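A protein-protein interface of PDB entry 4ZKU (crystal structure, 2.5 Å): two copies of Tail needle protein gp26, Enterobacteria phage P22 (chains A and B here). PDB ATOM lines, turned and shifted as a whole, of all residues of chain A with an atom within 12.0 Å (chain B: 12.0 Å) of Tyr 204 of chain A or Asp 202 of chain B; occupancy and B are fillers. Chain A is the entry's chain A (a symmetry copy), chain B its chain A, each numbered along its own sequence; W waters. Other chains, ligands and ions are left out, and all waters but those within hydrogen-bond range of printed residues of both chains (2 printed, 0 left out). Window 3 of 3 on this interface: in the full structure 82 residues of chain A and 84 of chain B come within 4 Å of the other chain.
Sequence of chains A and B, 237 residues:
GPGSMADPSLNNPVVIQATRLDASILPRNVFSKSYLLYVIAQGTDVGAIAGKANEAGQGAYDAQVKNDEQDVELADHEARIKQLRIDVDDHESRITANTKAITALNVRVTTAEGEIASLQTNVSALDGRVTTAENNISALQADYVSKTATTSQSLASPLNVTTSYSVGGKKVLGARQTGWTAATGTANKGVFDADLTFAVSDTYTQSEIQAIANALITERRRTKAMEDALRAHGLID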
ATOM      1  N   ALA A 199     -15.842  -8.117  25.452  1.00  0.00           N
ATOM      2  CA  ALA A 199     -15.157  -7.155  24.602  1.00  0.00           C
ATOM      3  C   ALA A 199     -14.095  -7.868  23.776  1.00  0.00           C
ATOM      4  O   ALA A 199     -13.354  -8.704  24.292  1.00  0.00           O
ATOM      5  CB  ALA A 199     -14.535  -6.051  25.439  1.00  0.00           C
ATOM      6  N   VAL A 200     -14.025  -7.536  22.490  1.00  0.00           N
ATOM      7  CA  VAL A 200     -13.009  -8.092  21.603  1.00  0.00           C
ATOM      8  C   VAL A 200     -12.367  -6.965  20.808  1.00  0.00           C
ATOM      9  O   VAL A 200     -12.996  -6.369  19.933  1.00  0.00           O
ATOM     10  CB  VAL A 200     -13.592  -9.162  20.655  1.00  0.00           C
ATOM     11  CG1 VAL A 200     -12.481  -9.796  19.831  1.00  0.00           C
ATOM     12  CG2 VAL A 200     -14.350 -10.228  21.437  1.00  0.00           C
ATOM     13  N   SER A 201     -11.109  -6.675  21.125  1.00  0.00           N
ATOM     14  CA  SER A 201     -10.388  -5.579  20.488  1.00  0.00           C
ATOM     15  C   SER A 201      -9.799  -5.970  19.139  1.00  0.00           C
ATOM     16  O   SER A 201      -9.780  -7.145  18.773  1.00  0.00           O
ATOM     17  CB  SER A 201      -9.267  -5.091  21.406  1.00  0.00           C
ATOM     18  OG  SER A 201      -9.780  -4.701  22.668  1.00  0.00           O
ATOM     19  N   ASP A 202      -9.322  -4.971  18.403  1.00  0.00           N
ATOM     20  CA  ASP A 202      -8.612  -5.207  17.152  1.00  0.00           C
ATOM     21  C   ASP A 202      -7.236  -5.802  17.429  1.00  0.00           C
ATOM     22  O   ASP A 202      -6.654  -6.477  16.581  1.00  0.00           O
ATOM     23  CB  ASP A 202      -8.476  -3.910  16.353  1.00  0.00           C
ATOM     24  CG  ASP A 202      -8.044  -2.738  17.212  1.00  0.00           C
ATOM     25  OD1 ASP A 202      -8.750  -2.429  18.195  1.00  0.00           O
ATOM     26  OD2 ASP A 202      -6.999  -2.128  16.901  1.00  0.00           O
ATOM     27  N   THR A 203      -6.723  -5.541  18.628  1.00  0.00           N
ATOM     28  CA  THR A 203      -5.417  -6.039  19.041  1.00  0.00           C
ATOM     29  C   THR A 203      -5.549  -7.004  20.212  1.00  0.00           C
ATOM     30  O   THR A 203      -6.527  -6.952  20.959  1.00  0.00           O
ATOM     31  CB  THR A 203      -4.476  -4.888  19.435  1.00  0.00           C
ATOM     32  OG1 THR A 203      -5.042  -4.160  20.533  1.00  0.00           O
ATOM     33  CG2 THR A 203      -4.266  -3.945  18.261  1.00  0.00           C
ATOM     34  N   TYR A 204      -4.569  -7.890  20.361  1.00  0.00           N
ATOM     35  CA  TYR A 204      -4.597  -8.893  21.423  1.00  0.00           C
ATOM     36  C   TYR A 204      -4.619  -8.253  22.808  1.00  0.00           C
ATOM     37  O   TYR A 204      -3.771  -7.424  23.138  1.00  0.00           O
ATOM     38  CB  TYR A 204      -3.398  -9.837  21.308  1.00  0.00           C
ATOM     39  CG  TYR A 204      -3.365 -10.904  22.382  1.00  0.00           C
ATOM     40  CD1 TYR A 204      -4.087 -12.082  22.238  1.00  0.00           C
ATOM     41  CD2 TYR A 204      -2.614 -10.734  23.540  1.00  0.00           C
ATOM     42  CE1 TYR A 204      -4.063 -13.059  23.215  1.00  0.00           C
ATOM     43  CE2 TYR A 204      -2.587 -11.706  24.524  1.00  0.00           C
ATOM     44  CZ  TYR A 204      -3.312 -12.867  24.354  1.00  0.00           C
ATOM     45  OH  TYR A 204      -3.288 -13.841  25.327  1.00  0.00           O
ATOM     46  N   THR A 205      -5.602  -8.647  23.611  1.00  0.00           N
ATOM     47  CA  THR A 205      -5.751  -8.139  24.967  1.00  0.00           C
ATOM     48  C   THR A 205      -5.909  -9.304  25.937  1.00  0.00           C
ATOM     49  O   THR A 205      -6.908 -10.024  25.886  1.00  0.00           O
ATOM     50  CB  THR A 205      -6.961  -7.196  25.090  1.00  0.00           C
ATOM     51  OG1 THR A 205      -6.945  -6.252  24.011  1.00  0.00           O
ATOM     52  CG2 THR A 205      -6.925  -6.447  26.413  1.00  0.00           C
ATOM     53  N   GLN A 206      -4.915  -9.498  26.802  1.00  0.00           N
ATOM     54  CA  GLN A 206      -4.898 -10.631  27.726  1.00  0.00           C
ATOM     55  C   GLN A 206      -6.164 -10.703  28.573  1.00  0.00           C
ATOM     56  O   GLN A 206      -6.754 -11.770  28.732  1.00  0.00           O
ATOM     57  CB  GLN A 206      -3.676 -10.560  28.645  1.00  0.00           C
ATOM     58  CG  GLN A 206      -3.612 -11.694  29.661  1.00  0.00           C
ATOM     59  CD  GLN A 206      -2.419 -11.589  30.590  1.00  0.00           C
ATOM     60  OE1 GLN A 206      -2.163 -10.536  31.173  1.00  0.00           O
ATOM     61  NE2 GLN A 206      -1.685 -12.685  30.736  1.00  0.00           N
ATOM     62  N   SER A 207      -6.572  -9.560  29.117  1.00  0.00           N
ATOM     63  CA  SER A 207      -7.722  -9.492  30.012  1.00  0.00           C
ATOM     64  C   SER A 207      -9.016  -9.887  29.308  1.00  0.00           C
ATOM     65  O   SER A 207      -9.914 -10.464  29.924  1.00  0.00           O
ATOM     66  CB  SER A 207      -7.855  -8.085  30.598  1.00  0.00           C
ATOM     67  OG  SER A 207      -8.140  -7.133  29.586  1.00  0.00           O
ATOM     68  N   GLU A 208      -9.108  -9.575  28.019  1.00  0.00           N
ATOM     69  CA  GLU A 208     -10.293  -9.920  27.237  1.00  0.00           C
ATOM     70  C   GLU A 208     -10.366 -11.424  26.993  1.00  0.00           C
ATOM     71  O   GLU A 208     -11.447 -12.011  26.993  1.00  0.00           O
ATOM     72  CB  GLU A 208     -10.299  -9.172  25.898  1.00  0.00           C
ATOM     73  CG  GLU A 208     -10.481  -7.663  26.022  1.00  0.00           C
ATOM     74  CD  GLU A 208     -10.499  -6.968  24.692  1.00  0.00           C
ATOM     75  OE1 GLU A 208     -10.146  -7.605  23.680  1.00  0.00           O
ATOM     76  OE2 GLU A 208     -10.856  -5.772  24.648  1.00  0.00           O
ATOM     77  N   ILE A 209      -9.209 -12.044  26.777  1.00  0.00           N
ATOM     78  CA  ILE A 209      -9.136 -13.480  26.548  1.00  0.00           C
ATOM     79  C   ILE A 209      -9.374 -14.209  27.866  1.00  0.00           C
ATOM     80  O   ILE A 209      -9.980 -15.280  27.896  1.00  0.00           O
ATOM     81  CB  ILE A 209      -7.785 -13.878  25.923  1.00  0.00           C
ATOM     82  CG1 ILE A 209      -7.539 -13.086  24.638  1.00  0.00           C
ATOM     83  CG2 ILE A 209      -7.740 -15.371  25.642  1.00  0.00           C
ATOM     84  CD1 ILE A 209      -8.519 -13.411  23.529  1.00  0.00           C
ATOM     85  N   GLN A 210      -8.897 -13.614  28.957  1.00  0.00           N
ATOM     86  CA  GLN A 210      -9.094 -14.169  30.293  1.00  0.00           C
ATOM     87  C   GLN A 210     -10.573 -14.208  30.662  1.00  0.00           C
ATOM     88  O   GLN A 210     -11.047 -15.172  31.265  1.00  0.00           O
ATOM     89  CB  GLN A 210      -8.321 -13.355  31.334  1.00  0.00           C
ATOM     90  CG  GLN A 210      -6.830 -13.641  31.370  1.00  0.00           C
ATOM     91  CD  GLN A 210      -6.076 -12.683  32.272  1.00  0.00           C
ATOM     92  OE1 GLN A 210      -6.527 -11.565  32.524  1.00  0.00           O
ATOM     93  NE2 GLN A 210      -4.920 -13.115  32.762  1.00  0.00           N
ATOM     94  N   ALA A 211     -11.293 -13.151  30.301  1.00  0.00           N
ATOM     95  CA  ALA A 211     -12.722 -13.057  30.576  1.00  0.00           C
ATOM     96  C   ALA A 211     -13.489 -14.164  29.861  1.00  0.00           C
ATOM     97  O   ALA A 211     -14.381 -14.788  30.438  1.00  0.00           O
ATOM     98  CB  ALA A 211     -13.254 -11.693  30.167  1.00  0.00           C
ATOM     99  N   ILE A 212     -13.139 -14.393  28.600  1.00  0.00           N
ATOM    100  CA  ILE A 212     -13.750 -15.450  27.803  1.00  0.00           C
ATOM    101  C   ILE A 212     -13.495 -16.813  28.440  1.00  0.00           C
ATOM    102  O   ILE A 212     -14.407 -17.629  28.563  1.00  0.00           O
ATOM    103  CB  ILE A 212     -13.234 -15.414  26.352  1.00  0.00           C
ATOM    104  CG1 ILE A 212     -13.784 -14.186  25.624  1.00  0.00           C
ATOM    105  CG2 ILE A 212     -13.614 -16.688  25.615  1.00  0.00           C
ATOM    106  CD1 ILE A 212     -13.176 -13.965  24.255  1.00  0.00           C
ATOM    107  N   ALA A 213     -12.252 -17.047  28.846  1.00  0.00           N
ATOM    108  CA  ALA A 213     -11.874 -18.308  29.472  1.00  0.00           C
ATOM    109  C   ALA A 213     -12.589 -18.494  30.805  1.00  0.00           C
ATOM    110  O   ALA A 213     -13.046 -19.590  31.126  1.00  0.00           O
ATOM    111  CB  ALA A 213     -10.366 -18.376  29.663  1.00  0.00           C
ATOM    112  N   ASN A 214     -12.676 -17.416  31.579  1.00  0.00           N
ATOM    113  CA  ASN A 214     -13.336 -17.448  32.880  1.00  0.00           C
ATOM    114  C   ASN A 214     -14.810 -17.817  32.751  1.00  0.00           C
ATOM    115  O   ASN A 214     -15.340 -18.580  33.558  1.00  0.00           O
ATOM    116  CB  ASN A 214     -13.195 -16.096  33.585  1.00  0.00           C
ATOM    117  CG  ASN A 214     -11.828 -15.904  34.212  1.00  0.00           C
ATOM    118  OD1 ASN A 214     -10.980 -16.796  34.162  1.00  0.00           O
ATOM    119  ND2 ASN A 214     -11.610 -14.740  34.810  1.00  0.00           N
ATOM    120  N   PHE B 198      -7.358 -22.693  31.756  1.00  0.00           N
ATOM    121  CA  PHE B 198      -6.659 -22.282  30.545  1.00  0.00           C
ATOM    122  C   PHE B 198      -5.565 -21.254  30.799  1.00  0.00           C
ATOM    123  O   PHE B 198      -5.748 -20.306  31.564  1.00  0.00           O
ATOM    124  CB  PHE B 198      -7.660 -21.725  29.534  1.00  0.00           C
ATOM    125  CG  PHE B 198      -8.873 -22.586  29.356  1.00  0.00           C
ATOM    126  CD1 PHE B 198      -8.844 -23.670  28.496  1.00  0.00           C
ATOM    127  CD2 PHE B 198     -10.036 -22.324  30.060  1.00  0.00           C
ATOM    128  CE1 PHE B 198      -9.950 -24.469  28.338  1.00  0.00           C
ATOM    129  CE2 PHE B 198     -11.150 -23.121  29.904  1.00  0.00           C
ATOM    130  CZ  PHE B 198     -11.105 -24.195  29.044  1.00  0.00           C
ATOM    131  N   ALA B 199      -4.423 -21.457  30.150  1.00  0.00           N
ATOM    132  CA  ALA B 199      -3.331 -20.498  30.207  1.00  0.00           C
ATOM    133  C   ALA B 199      -3.630 -19.327  29.279  1.00  0.00           C
ATOM    134  O   ALA B 199      -4.075 -19.521  28.147  1.00  0.00           O
ATOM    135  CB  ALA B 199      -2.018 -21.160  29.829  1.00  0.00           C
ATOM    136  N   VAL B 200      -3.385 -18.113  29.761  1.00  0.00           N
ATOM    137  CA  VAL B 200      -3.561 -16.910  28.954  1.00  0.00           C
ATOM    138  C   VAL B 200      -2.329 -16.028  29.093  1.00  0.00           C
ATOM    139  O   VAL B 200      -2.085 -15.443  30.150  1.00  0.00           O
ATOM    140  CB  VAL B 200      -4.835 -16.133  29.346  1.00  0.00           C
ATOM    141  CG1 VAL B 200      -5.041 -14.954  28.406  1.00  0.00           C
ATOM    142  CG2 VAL B 200      -6.056 -17.043  29.334  1.00  0.00           C
ATOM    143  N   SER B 201      -1.553 -15.940  28.019  1.00  0.00           N
ATOM    144  CA  SER B 201      -0.309 -15.180  28.027  1.00  0.00           C
ATOM    145  C   SER B 201      -0.530 -13.691  27.801  1.00  0.00           C
ATOM    146  O   SER B 201      -1.627 -13.261  27.446  1.00  0.00           O
ATOM    147  CB  SER B 201       0.638 -15.719  26.955  1.00  0.00           C
ATOM    148  OG  SER B 201       0.882 -17.101  27.141  1.00  0.00           O
ATOM    149  N   ASP B 202       0.523 -12.909  28.014  1.00  0.00           N
ATOM    150  CA  ASP B 202       0.497 -11.483  27.713  1.00  0.00           C
ATOM    151  C   ASP B 202       0.505 -11.262  26.205  1.00  0.00           C
ATOM    152  O   ASP B 202       0.052 -10.227  25.713  1.00  0.00           O
ATOM    153  CB  ASP B 202       1.687 -10.770  28.358  1.00  0.00           C
ATOM    154  CG  ASP B 202       2.991 -11.520  28.164  1.00  0.00           C
ATOM    155  OD1 ASP B 202       3.067 -12.697  28.576  1.00  0.00           O
ATOM    156  OD2 ASP B 202       3.937 -10.931  27.599  1.00  0.00           O
ATOM    157  N   THR B 203       1.025 -12.246  25.478  1.00  0.00           N
ATOM    158  CA  THR B 203       1.103 -12.181  24.023  1.00  0.00           C
ATOM    159  C   THR B 203       0.244 -13.265  23.385  1.00  0.00           C
ATOM    160  O   THR B 203      -0.037 -14.289  24.009  1.00  0.00           O
ATOM    161  CB  THR B 203       2.553 -12.327  23.531  1.00  0.00           C
ATOM    162  OG1 THR B 203       3.076 -13.594  23.950  1.00  0.00           O
ATOM    163  CG2 THR B 203       3.420 -11.213  24.095  1.00  0.00           C
ATOM    164  N   TYR B 204      -0.180 -13.032  22.146  1.00  0.00           N
ATOM    165  CA  TYR B 204      -1.040 -13.976  21.439  1.00  0.00           C
ATOM    166  C   TYR B 204      -0.366 -15.334  21.260  1.00  0.00           C
ATOM    167  O   TYR B 204       0.747 -15.427  20.744  1.00  0.00           O
ATOM    168  CB  TYR B 204      -1.449 -13.418  20.074  1.00  0.00           C
ATOM    169  CG  TYR B 204      -2.344 -14.351  19.285  1.00  0.00           C
ATOM    170  CD1 TYR B 204      -3.716 -14.370  19.496  1.00  0.00           C
ATOM    171  CD2 TYR B 204      -1.817 -15.214  18.330  1.00  0.00           C
ATOM    172  CE1 TYR B 204      -4.539 -15.219  18.781  1.00  0.00           C
ATOM    173  CE2 TYR B 204      -2.634 -16.069  17.611  1.00  0.00           C
ATOM    174  CZ  TYR B 204      -3.993 -16.066  17.841  1.00  0.00           C
ATOM    175  OH  TYR B 204      -4.813 -16.911  17.128  1.00  0.00           O
ATOM    176  N   THR B 205      -1.057 -16.382  21.697  1.00  0.00           N
ATOM    177  CA  THR B 205      -0.555 -17.745  21.588  1.00  0.00           C
ATOM    178  C   THR B 205      -1.622 -18.634  20.957  1.00  0.00           C
ATOM    179  O   THR B 205      -2.675 -18.860  21.556  1.00  0.00           O
ATOM    180  CB  THR B 205      -0.150 -18.313  22.959  1.00  0.00           C
ATOM    181  OG1 THR B 205       0.650 -17.353  23.659  1.00  0.00           O
ATOM    182  CG2 THR B 205       0.641 -19.602  22.792  1.00  0.00           C
ATOM    183  N   GLN B 206      -1.354 -19.118  19.747  1.00  0.00           N
ATOM    184  CA  GLN B 206      -2.326 -19.910  18.994  1.00  0.00           C
ATOM    185  C   GLN B 206      -2.827 -21.113  19.786  1.00  0.00           C
ATOM    186  O   GLN B 206      -4.026 -21.381  19.828  1.00  0.00           O
ATOM    187  CB  GLN B 206      -1.724 -20.389  17.670  1.00  0.00           C
ATOM    188  CG  GLN B 206      -2.672 -21.251  16.847  1.00  0.00           C
ATOM    189  CD  GLN B 206      -2.050 -21.751  15.559  1.00  0.00           C
ATOM    190  OE1 GLN B 206      -0.942 -22.289  15.559  1.00  0.00           O
ATOM    191  NE2 GLN B 206      -2.761 -21.580  14.452  1.00  0.00           N
ATOM    192  N   SER B 207      -1.898 -21.834  20.407  1.00  0.00           N
ATOM    193  CA  SER B 207      -2.222 -23.054  21.138  1.00  0.00           C
ATOM    194  C   SER B 207      -3.136 -22.780  22.328  1.00  0.00           C
ATOM    195  O   SER B 207      -3.973 -23.612  22.680  1.00  0.00           O
ATOM    196  CB  SER B 207      -0.941 -23.744  21.611  1.00  0.00           C
ATOM    197  OG  SER B 207      -0.246 -22.944  22.553  1.00  0.00           O
ATOM    198  N   GLU B 208      -2.972 -21.613  22.944  1.00  0.00           N
ATOM    199  CA  GLU B 208      -3.803 -21.234  24.084  1.00  0.00           C
ATOM    200  C   GLU B 208      -5.230 -20.927  23.641  1.00  0.00           C
ATOM    201  O   GLU B 208      -6.189 -21.236  24.347  1.00  0.00           O
ATOM    202  CB  GLU B 208      -3.209 -20.021  24.811  1.00  0.00           C
ATOM    203  CG  GLU B 208      -1.884 -20.297  25.516  1.00  0.00           C
ATOM    204  CD  GLU B 208      -1.343 -19.094  26.229  1.00  0.00           C
ATOM    205  OE1 GLU B 208      -1.859 -17.982  26.002  1.00  0.00           O
ATOM    206  OE2 GLU B 208      -0.386 -19.246  27.016  1.00  0.00           O
ATOM    207  N   ILE B 209      -5.364 -20.309  22.471  1.00  0.00           N
ATOM    208  CA  ILE B 209      -6.672 -19.973  21.923  1.00  0.00           C
ATOM    209  C   ILE B 209      -7.344 -21.246  21.421  1.00  0.00           C
ATOM    210  O   ILE B 209      -8.561 -21.398  21.517  1.00  0.00           O
ATOM    211  CB  ILE B 209      -6.555 -18.921  20.804  1.00  0.00           C
ATOM    212  CG1 ILE B 209      -5.818 -17.681  21.312  1.00  0.00           C
ATOM    213  CG2 ILE B 209      -7.928 -18.542  20.275  1.00  0.00           C
ATOM    214  CD1 ILE B 209      -6.573 -16.928  22.390  1.00  0.00           C
ATOM    215  N   GLN B 210      -6.538 -22.161  20.889  1.00  0.00           N
ATOM    216  CA  GLN B 210      -7.034 -23.451  20.413  1.00  0.00           C
ATOM    217  C   GLN B 210      -7.619 -24.273  21.556  1.00  0.00           C
ATOM    218  O   GLN B 210      -8.649 -24.931  21.396  1.00  0.00           O
ATOM    219  CB  GLN B 210      -5.915 -24.238  19.727  1.00  0.00           C
ATOM    220  CG  GLN B 210      -5.596 -23.773  18.317  1.00  0.00           C
ATOM    221  CD  GLN B 210      -4.361 -24.445  17.749  1.00  0.00           C
ATOM    222  OE1 GLN B 210      -3.493 -24.903  18.491  1.00  0.00           O
ATOM    223  NE2 GLN B 210      -4.276 -24.507  16.425  1.00  0.00           N
ATOM    224  N   ALA B 211      -6.953 -24.234  22.705  1.00  0.00           N
ATOM    225  CA  ALA B 211      -7.403 -24.961  23.885  1.00  0.00           C
ATOM    226  C   ALA B 211      -8.766 -24.459  24.348  1.00  0.00           C
ATOM    227  O   ALA B 211      -9.648 -25.250  24.689  1.00  0.00           O
ATOM    228  CB  ALA B 211      -6.384 -24.837  25.007  1.00  0.00           C
ATOM    229  N   ILE B 212      -8.926 -23.140  24.363  1.00  0.00           N
ATOM    230  CA  ILE B 212     -10.189 -22.514  24.736  1.00  0.00           C
ATOM    231  C   ILE B 212     -11.299 -22.943  23.781  1.00  0.00           C
ATOM    232  O   ILE B 212     -12.396 -23.298  24.210  1.00  0.00           O
ATOM    233  CB  ILE B 212     -10.054 -20.980  24.772  1.00  0.00           C
ATOM    234  CG1 ILE B 212      -9.189 -20.551  25.959  1.00  0.00           C
ATOM    235  CG2 ILE B 212     -11.423 -20.321  24.842  1.00  0.00           C
ATOM    236  CD1 ILE B 212      -8.842 -19.078  25.960  1.00  0.00           C
HETATM  237  O   HOH W   1      -2.843 -15.213  32.900  1.00  0.00           O
HETATM  238  O   HOH W   2      -2.811 -16.414  24.410  1.00  0.00           O
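Water W2 lies within hydrogen-bond range of OE1 of Glu 208 of chain B (2.4 Å), OH of Tyr 204 of chain A (2.8 Å) and N of Thr 205 of chain B (3.2 Å). Water W1 lies within hydrogen-bond range of the backbone carbonyl oxygen of Val 200 of chain B (2.9 Å) and the side-chain amide nitrogen of Gln 210 of chain A (3.0 Å).
Tyr 204 of chain A touches Val 200 of chain B, but with the chains exchanged Val 200 of chain A does not touch Tyr 204 of chain B (9.7 Å). Tyr 204 of chain A touches Ser 201 of chain B, but with the chains exchanged Ser 201 of chain A does not touch Tyr 204 of chain B (9.5 Å). Ile 209 of chain A touches Val 200 of chain B, but with the chains exchanged Val 200 of chain A does not touch Ile 209 of chain B (9.6 Å). Gln 210 of chain A touches Val 200 of chain B, but with the chains exchanged Val 200 of chain A does not touch Gln 210 of chain B (13.8 Å). Positions printed for both chains: 199, 200, 201, 202, 203, 204, 205, 206, 207, 208, 209, 210, 211 and 212. Of the 13 pairs that touch across the chains among the printed residues, 2 have their exchanged pair printed and touching as well.
No residue of chain B comes within 4 Å of Ser 201 of chain A. Asp 202 of chain A touches none of the printed residues of chain B. No residue of chain B comes within 4 Å of Thr 203 of chain A. Tyr 204 of chain A touches just these residues of chain B: Val 200, Ser 201, Asp 202, Thr 203 and Tyr 204. Of chain B, only Val 200, Ser 201 and Asp 202 come within 4 Å of Gln 206 of chain A. Ser 207 of chain A touches none of the printed residues of chain B. Of the printed residues of chain B, Ile 209 of chain A touches Val 200 (3.9 Å), Ile 209 (3.8 Å) and Ile 212 (3.9 Å). Asn 214 of chain A touches none of the printed residues of chain B. Printed residues of chain A within 4 Å of Phe 198 of chain B: Ala 213. Ser 201 of chain B touches just these residues of chain A: Tyr 204 (2.8 Å) and Gln 206 (3.3 Å). Of the printed residues of chain A, Asp 202 of chain B touches Tyr 204 (3.3 Å) and Gln 206 (3.5 Å). Of chain A, only Tyr 204 comes within 4 Å of Tyr 204 of chain B. No residue of chain A comes within 4 Å of Thr 205 of chain B. Of the printed residues of chain A, Ile 212 of chain B touches Ile 209 (3.9 Å). The nearest residue of chain B that does not touch Tyr 204 of chain A is Glu 208 of chain B (4.4 Å).
Tyr 204 of chain A touches Val 200 of chain B. O of Asp 202 of chain B touches CE2 of Tyr 204 of chain A (3.3 Å). C of Thr 203 of chain B touches CE2 of Tyr 204 of chain A, 3.4 Å away. CD1 of Tyr 204 of chain A touches CD1 of Tyr 204 of chain B, at 3.6 Å. Gln 206 of chain A touches Asp 202 of chain B (NE2 to N, 3.5 Å). Val 200 of chain B touches Ile 209 of chain A. CG2 of Ile 209 of chain A touches CD1 of Ile 209 of chain B (3.8 Å). Ile 209 of chain A touches Ile 212 of chain B. Gln 210 of chain A touches Val 200 of chain B (CG to CG1, 3.7 Å). Ala 213 of chain A touches Phe 198 of chain B.
NE2 of Gln 206 of chain A lies within hydrogen-bond range of O of Val 200 of chain B, 2.8 Å away. The backbone carbonyl oxygen (O) of Ser 201 of chain B is in hydrogen-bond range of the side-chain hydroxyl (OH) of Tyr 204 of chain A, 2.8 Å away. The side-chain amide nitrogen (NE2) of Gln 206 of chain A lies close to the backbone carbonyl oxygen (O) of Ser 201 of chain B, 3.3 Å away.
The side-chain carboxylate (OE2) of Glu 208 of chain B lies within hydrogen-bond range of the side-chain hydroxyl (OG) of Ser 201 of chain B, at 2.5 Å. OG1 of Thr 205 of chain B lies within hydrogen-bond range of O of Thr 203 of chain B (3.2 Å). O of Gln 210 of chain A sits close to OD1 of Asn 214 of chain A. The side-chain hydroxyl (OG1) of Thr 205 of chain B sits at hydrogen-bond distance from the side-chain hydroxyl (OG) of Ser 201 of chain B (3.5 Å).
Hydrophobic or aromatic side chains of chain A that line the printed part of chain B: Tyr 204, Ile 209 and Ala 213. Along chain A the printed residues that touch a printed residue of chain B span positions 204 to 213. Hydrophobic or aromatic side chains of chain B within 4 Å of the printed part of chain A: Phe 198, Val 200, Tyr 204, Ile 209 and Ile 212. Among the printed residues, 13 pairs touch across the chains. Among the printed residues, no Asp or Glu carboxylate lies within 4 Å of a Lys or Arg side-chain nitrogen of the other chain.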
